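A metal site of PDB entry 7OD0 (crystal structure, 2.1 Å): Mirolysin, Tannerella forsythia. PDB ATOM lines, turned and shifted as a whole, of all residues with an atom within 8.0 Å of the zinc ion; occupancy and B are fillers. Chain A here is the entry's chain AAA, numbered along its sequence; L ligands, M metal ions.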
ATOM      1  N   GLY A 128     -16.523  -6.503  -8.095  1.00  0.00           N
ATOM      2  CA  GLY A 128     -15.988  -5.237  -8.624  1.00  0.00           C
ATOM      3  C   GLY A 128     -16.425  -4.078  -7.762  1.00  0.00           C
ATOM      4  O   GLY A 128     -17.262  -4.300  -6.838  1.00  0.00           O
ATOM      5  N   TYR A 129     -15.922  -2.888  -8.063  1.00  0.00           N
ATOM      6  CA  TYR A 129     -16.339  -1.645  -7.364  1.00  0.00           C
ATOM      7  C   TYR A 129     -16.128  -0.433  -8.264  1.00  0.00           C
ATOM      8  O   TYR A 129     -15.270  -0.453  -9.202  1.00  0.00           O
ATOM      9  CB  TYR A 129     -15.615  -1.519  -6.024  1.00  0.00           C
ATOM     10  CG  TYR A 129     -14.131  -1.225  -6.078  1.00  0.00           C
ATOM     11  CD1 TYR A 129     -13.215  -2.243  -6.214  1.00  0.00           C
ATOM     12  CD2 TYR A 129     -13.647   0.059  -5.918  1.00  0.00           C
ATOM     13  CE1 TYR A 129     -11.860  -1.991  -6.225  1.00  0.00           C
ATOM     14  CE2 TYR A 129     -12.295   0.334  -5.939  1.00  0.00           C
ATOM     15  CZ  TYR A 129     -11.387  -0.696  -6.078  1.00  0.00           C
ATOM     16  OH  TYR A 129     -10.052  -0.462  -6.102  1.00  0.00           O
ATOM     17  N   ALA A 130     -16.932   0.591  -7.971  1.00  0.00           N
ATOM     18  CA  ALA A 130     -16.995   1.861  -8.716  1.00  0.00           C
ATOM     19  C   ALA A 130     -16.554   3.017  -7.826  1.00  0.00           C
ATOM     20  O   ALA A 130     -16.419   2.811  -6.629  1.00  0.00           O
ATOM     21  CB  ALA A 130     -18.396   2.077  -9.210  1.00  0.00           C
ATOM     22  N   PHE A 132     -18.151   6.961  -7.293  1.00  0.00           N
ATOM     23  CA  PHE A 132     -19.290   7.860  -7.652  1.00  0.00           C
ATOM     24  C   PHE A 132     -18.756   9.211  -8.110  1.00  0.00           C
ATOM     25  O   PHE A 132     -17.690   9.643  -7.685  1.00  0.00           O
ATOM     26  CB  PHE A 132     -20.227   8.043  -6.454  1.00  0.00           C
ATOM     27  CG  PHE A 132     -21.031   6.812  -6.148  1.00  0.00           C
ATOM     28  CD1 PHE A 132     -22.164   6.526  -6.890  1.00  0.00           C
ATOM     29  CD2 PHE A 132     -20.685   5.956  -5.120  1.00  0.00           C
ATOM     30  CE1 PHE A 132     -22.921   5.399  -6.632  1.00  0.00           C
ATOM     31  CE2 PHE A 132     -21.451   4.831  -4.851  1.00  0.00           C
ATOM     32  CZ  PHE A 132     -22.568   4.561  -5.593  1.00  0.00           C
ATOM     33  N   THR A 167     -21.382  -7.355 -14.243  1.00  0.00           N
ATOM     34  CA  THR A 167     -20.633  -6.665 -13.158  1.00  0.00           C
ATOM     35  C   THR A 167     -20.233  -5.270 -13.653  1.00  0.00           C
ATOM     36  O   THR A 167     -20.489  -4.288 -12.916  1.00  0.00           O
ATOM     37  CB  THR A 167     -19.410  -7.469 -12.685  1.00  0.00           C
ATOM     38  OG1 THR A 167     -19.882  -8.763 -12.325  1.00  0.00           O
ATOM     39  CG2 THR A 167     -18.720  -6.819 -11.505  1.00  0.00           C
ATOM     40  N   HIS A 170     -23.257  -2.878 -14.091  1.00  0.00           N
ATOM     41  CA  HIS A 170     -23.661  -2.415 -12.744  1.00  0.00           C
ATOM     42  C   HIS A 170     -22.685  -1.317 -12.272  1.00  0.00           C
ATOM     43  O   HIS A 170     -23.146  -0.251 -11.803  1.00  0.00           O
ATOM     44  CB  HIS A 170     -23.748  -3.638 -11.818  1.00  0.00           C
ATOM     45  CG  HIS A 170     -24.002  -3.386 -10.369  1.00  0.00           C
ATOM     46  ND1 HIS A 170     -25.213  -3.710  -9.769  1.00  0.00           N
ATOM     47  CD2 HIS A 170     -23.193  -2.942  -9.381  1.00  0.00           C
ATOM     48  CE1 HIS A 170     -25.160  -3.420  -8.486  1.00  0.00           C
ATOM     49  NE2 HIS A 170     -23.915  -2.968  -8.210  1.00  0.00           N
ATOM     50  N   GLU A 171     -21.369  -1.558 -12.373  1.00  0.00           N
ATOM     51  CA  GLU A 171     -20.322  -0.614 -11.917  1.00  0.00           C
ATOM     52  C   GLU A 171     -20.334   0.653 -12.770  1.00  0.00           C
ATOM     53  O   GLU A 171     -20.167   1.763 -12.238  1.00  0.00           O
ATOM     54  CB  GLU A 171     -18.928  -1.259 -11.951  1.00  0.00           C
ATOM     55  CG  GLU A 171     -18.747  -2.419 -10.969  1.00  0.00           C
ATOM     56  CD  GLU A 171     -19.219  -2.221  -9.535  1.00  0.00           C
ATOM     57  OE1 GLU A 171     -19.376  -1.049  -9.097  1.00  0.00           O
ATOM     58  OE2 GLU A 171     -19.388  -3.267  -8.843  1.00  0.00           O
ATOM     59  N   GLY A 173     -22.913   1.812 -14.168  1.00  0.00           N
ATOM     60  CA  GLY A 173     -24.117   2.416 -13.542  1.00  0.00           C
ATOM     61  C   GLY A 173     -23.769   3.338 -12.362  1.00  0.00           C
ATOM     62  O   GLY A 173     -24.208   4.502 -12.370  1.00  0.00           O
ATOM     63  N   HIS A 174     -23.039   2.856 -11.367  1.00  0.00           N
ATOM     64  CA  HIS A 174     -22.611   3.628 -10.177  1.00  0.00           C
ATOM     65  C   HIS A 174     -21.733   4.827 -10.602  1.00  0.00           C
ATOM     66  O   HIS A 174     -21.906   5.941 -10.074  1.00  0.00           O
ATOM     67  CB  HIS A 174     -21.813   2.731  -9.208  1.00  0.00           C
ATOM     68  CG  HIS A 174     -22.625   1.780  -8.390  1.00  0.00           C
ATOM     69  ND1 HIS A 174     -23.813   2.147  -7.786  1.00  0.00           N
ATOM     70  CD2 HIS A 174     -22.369   0.517  -8.001  1.00  0.00           C
ATOM     71  CE1 HIS A 174     -24.279   1.126  -7.085  1.00  0.00           C
ATOM     72  NE2 HIS A 174     -23.404   0.111  -7.199  1.00  0.00           N
ATOM     73  N   LEU A 178     -25.838   6.067 -10.529  1.00  0.00           N
ATOM     74  CA  LEU A 178     -27.009   5.236 -10.128  1.00  0.00           C
ATOM     75  C   LEU A 178     -26.751   4.591  -8.776  1.00  0.00           C
ATOM     76  O   LEU A 178     -25.633   4.056  -8.566  1.00  0.00           O
ATOM     77  CB  LEU A 178     -27.281   4.161 -11.173  1.00  0.00           C
ATOM     78  CG  LEU A 178     -27.718   4.669 -12.547  1.00  0.00           C
ATOM     79  CD1 LEU A 178     -28.195   3.518 -13.403  1.00  0.00           C
ATOM     80  CD2 LEU A 178     -28.786   5.737 -12.427  1.00  0.00           C
ATOM     81  N   ARG A 179     -27.784   4.581  -7.917  1.00  0.00           N
ATOM     82  CA  ARG A 179     -27.738   3.894  -6.606  1.00  0.00           C
ATOM     83  C   ARG A 179     -28.412   2.522  -6.724  1.00  0.00           C
ATOM     84  O   ARG A 179     -29.238   2.313  -7.615  1.00  0.00           O
ATOM     85  CB  ARG A 179     -28.429   4.755  -5.540  1.00  0.00           C
ATOM     86  CG  ARG A 179     -27.804   6.133  -5.331  1.00  0.00           C
ATOM     87  CD  ARG A 179     -26.271   6.141  -5.274  1.00  0.00           C
ATOM     88  NE  ARG A 179     -25.607   6.971  -4.250  1.00  0.00           N
ATOM     89  CZ  ARG A 179     -24.882   8.073  -4.471  1.00  0.00           C
ATOM     90  NH1 ARG A 179     -24.748   8.572  -5.701  1.00  0.00           N
ATOM     91  NH2 ARG A 179     -24.299   8.681  -3.452  1.00  0.00           N
ATOM     92  N   HIS A 180     -28.057   1.616  -5.819  1.00  0.00           N
ATOM     93  CA  HIS A 180     -28.761   0.334  -5.593  1.00  0.00           C
ATOM     94  C   HIS A 180     -30.274   0.580  -5.553  1.00  0.00           C
ATOM     95  O   HIS A 180     -30.732   1.493  -4.810  1.00  0.00           O
ATOM     96  CB  HIS A 180     -28.268  -0.358  -4.308  1.00  0.00           C
ATOM     97  CG  HIS A 180     -26.858  -0.820  -4.423  1.00  0.00           C
ATOM     98  ND1 HIS A 180     -25.994  -0.808  -3.370  1.00  0.00           N
ATOM     99  CD2 HIS A 180     -26.180  -1.340  -5.477  1.00  0.00           C
ATOM    100  CE1 HIS A 180     -24.836  -1.297  -3.741  1.00  0.00           C
ATOM    101  NE2 HIS A 180     -24.913  -1.639  -5.030  1.00  0.00           N
ATOM    102  N   ILE A 181     -31.005  -0.232  -6.321  1.00  0.00           N
ATOM    103  CA  ILE A 181     -32.456  -0.061  -6.563  1.00  0.00           C
ATOM    104  C   ILE A 181     -33.216  -0.148  -5.241  1.00  0.00           C
ATOM    105  O   ILE A 181     -34.300   0.462  -5.172  1.00  0.00           O
ATOM    106  CB  ILE A 181     -32.960  -1.095  -7.595  1.00  0.00           C
ATOM    107  CG1 ILE A 181     -34.397  -0.803  -8.027  1.00  0.00           C
ATOM    108  CG2 ILE A 181     -32.795  -2.509  -7.067  1.00  0.00           C
ATOM    109  CD1 ILE A 181     -34.813  -1.569  -9.238  1.00  0.00           C
ATOM    110  N   TRP A 182     -32.695  -0.869  -4.234  1.00  0.00           N
ATOM    111  CA  TRP A 182     -33.387  -1.080  -2.931  1.00  0.00           C
ATOM    112  C   TRP A 182     -33.057   0.082  -1.957  1.00  0.00           C
ATOM    113  O   TRP A 182     -33.685   0.160  -0.888  1.00  0.00           O
ATOM    114  CB  TRP A 182     -33.035  -2.471  -2.358  1.00  0.00           C
ATOM    115  CG  TRP A 182     -31.633  -2.607  -1.878  1.00  0.00           C
ATOM    116  CD1 TRP A 182     -31.203  -2.366  -0.612  1.00  0.00           C
ATOM    117  CD2 TRP A 182     -30.477  -3.020  -2.615  1.00  0.00           C
ATOM    118  NE1 TRP A 182     -29.847  -2.566  -0.514  1.00  0.00           N
ATOM    119  CE2 TRP A 182     -29.379  -2.975  -1.733  1.00  0.00           C
ATOM    120  CE3 TRP A 182     -30.242  -3.434  -3.934  1.00  0.00           C
ATOM    121  CZ2 TRP A 182     -28.077  -3.305  -2.140  1.00  0.00           C
ATOM    122  CZ3 TRP A 182     -28.956  -3.748  -4.331  1.00  0.00           C
ATOM    123  CH2 TRP A 182     -27.897  -3.707  -3.434  1.00  0.00           C
ATOM    124  N   ASP A 184     -30.060   0.941  -0.409  1.00  0.00           N
ATOM    125  CA  ASP A 184     -28.934   0.816   0.559  1.00  0.00           C
ATOM    126  C   ASP A 184     -29.464   1.065   1.976  1.00  0.00           C
ATOM    127  O   ASP A 184     -28.842   1.822   2.730  1.00  0.00           O
ATOM    128  CB  ASP A 184     -27.794   1.797   0.183  1.00  0.00           C
ATOM    129  CG  ASP A 184     -27.119   1.414  -1.111  1.00  0.00           C
ATOM    130  OD1 ASP A 184     -26.752   0.223  -1.218  1.00  0.00           O
ATOM    131  OD2 ASP A 184     -26.987   2.270  -2.003  1.00  0.00           O
ATOM    132  N   TYR A 229     -30.285  -3.790 -13.617  1.00  0.00           N
ATOM    133  CA  TYR A 229     -28.809  -3.946 -13.523  1.00  0.00           C
ATOM    134  C   TYR A 229     -28.285  -3.549 -12.133  1.00  0.00           C
ATOM    135  O   TYR A 229     -27.242  -4.093 -11.743  1.00  0.00           O
ATOM    136  CB  TYR A 229     -28.097  -3.136 -14.601  1.00  0.00           C
ATOM    137  CG  TYR A 229     -28.440  -3.601 -15.983  1.00  0.00           C
ATOM    138  CD1 TYR A 229     -28.246  -4.921 -16.342  1.00  0.00           C
ATOM    139  CD2 TYR A 229     -28.971  -2.728 -16.920  1.00  0.00           C
ATOM    140  CE1 TYR A 229     -28.551  -5.369 -17.619  1.00  0.00           C
ATOM    141  CE2 TYR A 229     -29.306  -3.159 -18.188  1.00  0.00           C
ATOM    142  CZ  TYR A 229     -29.119  -4.491 -18.521  1.00  0.00           C
ATOM    143  OH  TYR A 229     -29.431  -4.951 -19.770  1.00  0.00           O
ATOM    144  N   MET A 230     -28.991  -2.656 -11.430  1.00  0.00           N
ATOM    145  CA  MET A 230     -28.517  -2.085 -10.148  1.00  0.00           C
ATOM    146  C   MET A 230     -29.032  -2.925  -8.952  1.00  0.00           C
ATOM    147  O   MET A 230     -28.961  -2.442  -7.819  1.00  0.00           O
ATOM    148  CB  MET A 230     -28.968  -0.628 -10.031  1.00  0.00           C
ATOM    149  CG  MET A 230     -28.481   0.228 -11.160  1.00  0.00           C
ATOM    150  SD  MET A 230     -26.728  -0.009 -11.580  1.00  0.00           S
ATOM    151  CE  MET A 230     -25.947   0.459 -10.041  1.00  0.00           C
ATOM    152  N   ASP A 231     -29.518  -4.145  -9.181  1.00  0.00           N
ATOM    153  CA  ASP A 231     -29.767  -5.119  -8.087  1.00  0.00           C
ATOM    154  C   ASP A 231     -28.540  -6.025  -7.977  1.00  0.00           C
ATOM    155  O   ASP A 231     -27.523  -5.749  -8.669  1.00  0.00           O
ATOM    156  CB  ASP A 231     -31.086  -5.856  -8.285  1.00  0.00           C
ATOM    157  CG  ASP A 231     -31.718  -6.266  -6.964  1.00  0.00           C
ATOM    158  OD1 ASP A 231     -30.983  -6.342  -5.951  1.00  0.00           O
ATOM    159  OD2 ASP A 231     -32.924  -6.546  -6.947  1.00  0.00           O
ATOM    160  N   TYR A 232     -28.596  -7.040  -7.124  1.00  0.00           N
ATOM    161  CA  TYR A 232     -27.438  -7.943  -6.893  1.00  0.00           C
ATOM    162  C   TYR A 232     -27.718  -9.339  -7.469  1.00  0.00           C
ATOM    163  O   TYR A 232     -27.115 -10.334  -7.015  1.00  0.00           O
ATOM    164  CB  TYR A 232     -27.135  -7.967  -5.398  1.00  0.00           C
ATOM    165  CG  TYR A 232     -26.186  -6.922  -4.885  1.00  0.00           C
ATOM    166  CD1 TYR A 232     -25.380  -6.156  -5.709  1.00  0.00           C
ATOM    167  CD2 TYR A 232     -26.013  -6.788  -3.505  1.00  0.00           C
ATOM    168  CE1 TYR A 232     -24.453  -5.266  -5.180  1.00  0.00           C
ATOM    169  CE2 TYR A 232     -25.137  -5.867  -2.971  1.00  0.00           C
ATOM    170  CZ  TYR A 232     -24.337  -5.120  -3.805  1.00  0.00           C
ATOM    171  OH  TYR A 232     -23.426  -4.245  -3.275  1.00  0.00           O
HETATM  172  C1  LIG L   1     -21.042  -2.372  -5.525  1.00  0.00           C
HETATM  173  O1  LIG L   1     -22.162  -2.679  -5.111  1.00  0.00           O
HETATM  174  O2  LIG L   1     -20.622  -2.712  -6.632  1.00  0.00           O
HETATM  175  C2  LIG L   1     -20.153  -1.474  -4.651  1.00  0.00           C
HETATM  176  N1  LG2 L   2     -25.087  -8.370 -10.215  1.00  0.00           N
HETATM  177  C1  LG2 L   2     -24.241  -7.162 -10.253  1.00  0.00           C
HETATM  178  C2  LG2 L   2     -23.232  -7.047  -9.131  1.00  0.00           C
HETATM  179  C3  LG2 L   2     -22.160  -6.153  -9.212  1.00  0.00           C
HETATM  180  C4  LG2 L   2     -21.244  -6.004  -8.184  1.00  0.00           C
HETATM  181  C5  LG2 L   2     -21.320  -6.733  -7.036  1.00  0.00           C
HETATM  182  C6  LG2 L   2     -22.395  -7.654  -6.912  1.00  0.00           C
HETATM  183  N2  LG2 L   2     -22.637  -8.473  -5.867  1.00  0.00           N
HETATM  184  S1  LG2 L   2     -23.824  -9.455  -6.359  1.00  0.00           S
HETATM  185  N3  LG2 L   2     -24.289  -8.724  -7.728  1.00  0.00           N
HETATM  186  C7  LG2 L   2     -23.345  -7.795  -7.982  1.00  0.00           C
HETATM  187 ZN    ZN M   1     -23.437  -1.893  -6.570  1.00  0.00          ZN
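Residues that only touch the zinc ion: Tyr 232.
Of the 19 residues printed, 4 come within 4 Å of the zinc ion.
The nearest printed residue that does not touch the zinc ion is Glu 171 (4.8 Å).
The zinc ion is bound by NE2 of His 170 (2.0 Å), O1 of LIG L1 (2.1 Å), NE2 of His 174 (2.1 Å) and NE2 of His 180 (2.1 Å).
The zinc ion has four donor atoms within binding distance.
A ring nitrogen (ND1) of His 174 sits at hydrogen-bond distance from the backbone carbonyl oxygen (O) of Leu 178 (2.8 Å).
NE2 of His 180 lies close to OH of Tyr 232.
O of Asp 231 lies within hydrogen-bond range of ND1 of His 170 (3.3 Å).
A ring nitrogen (ND1) of His 170 is in hydrogen-bond range of the backbone carbonyl oxygen (O) of Tyr 229 (2.9 Å).
A ring nitrogen (ND1) of His 180 is in hydrogen-bond range of the side-chain carboxylate of Asp 184.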
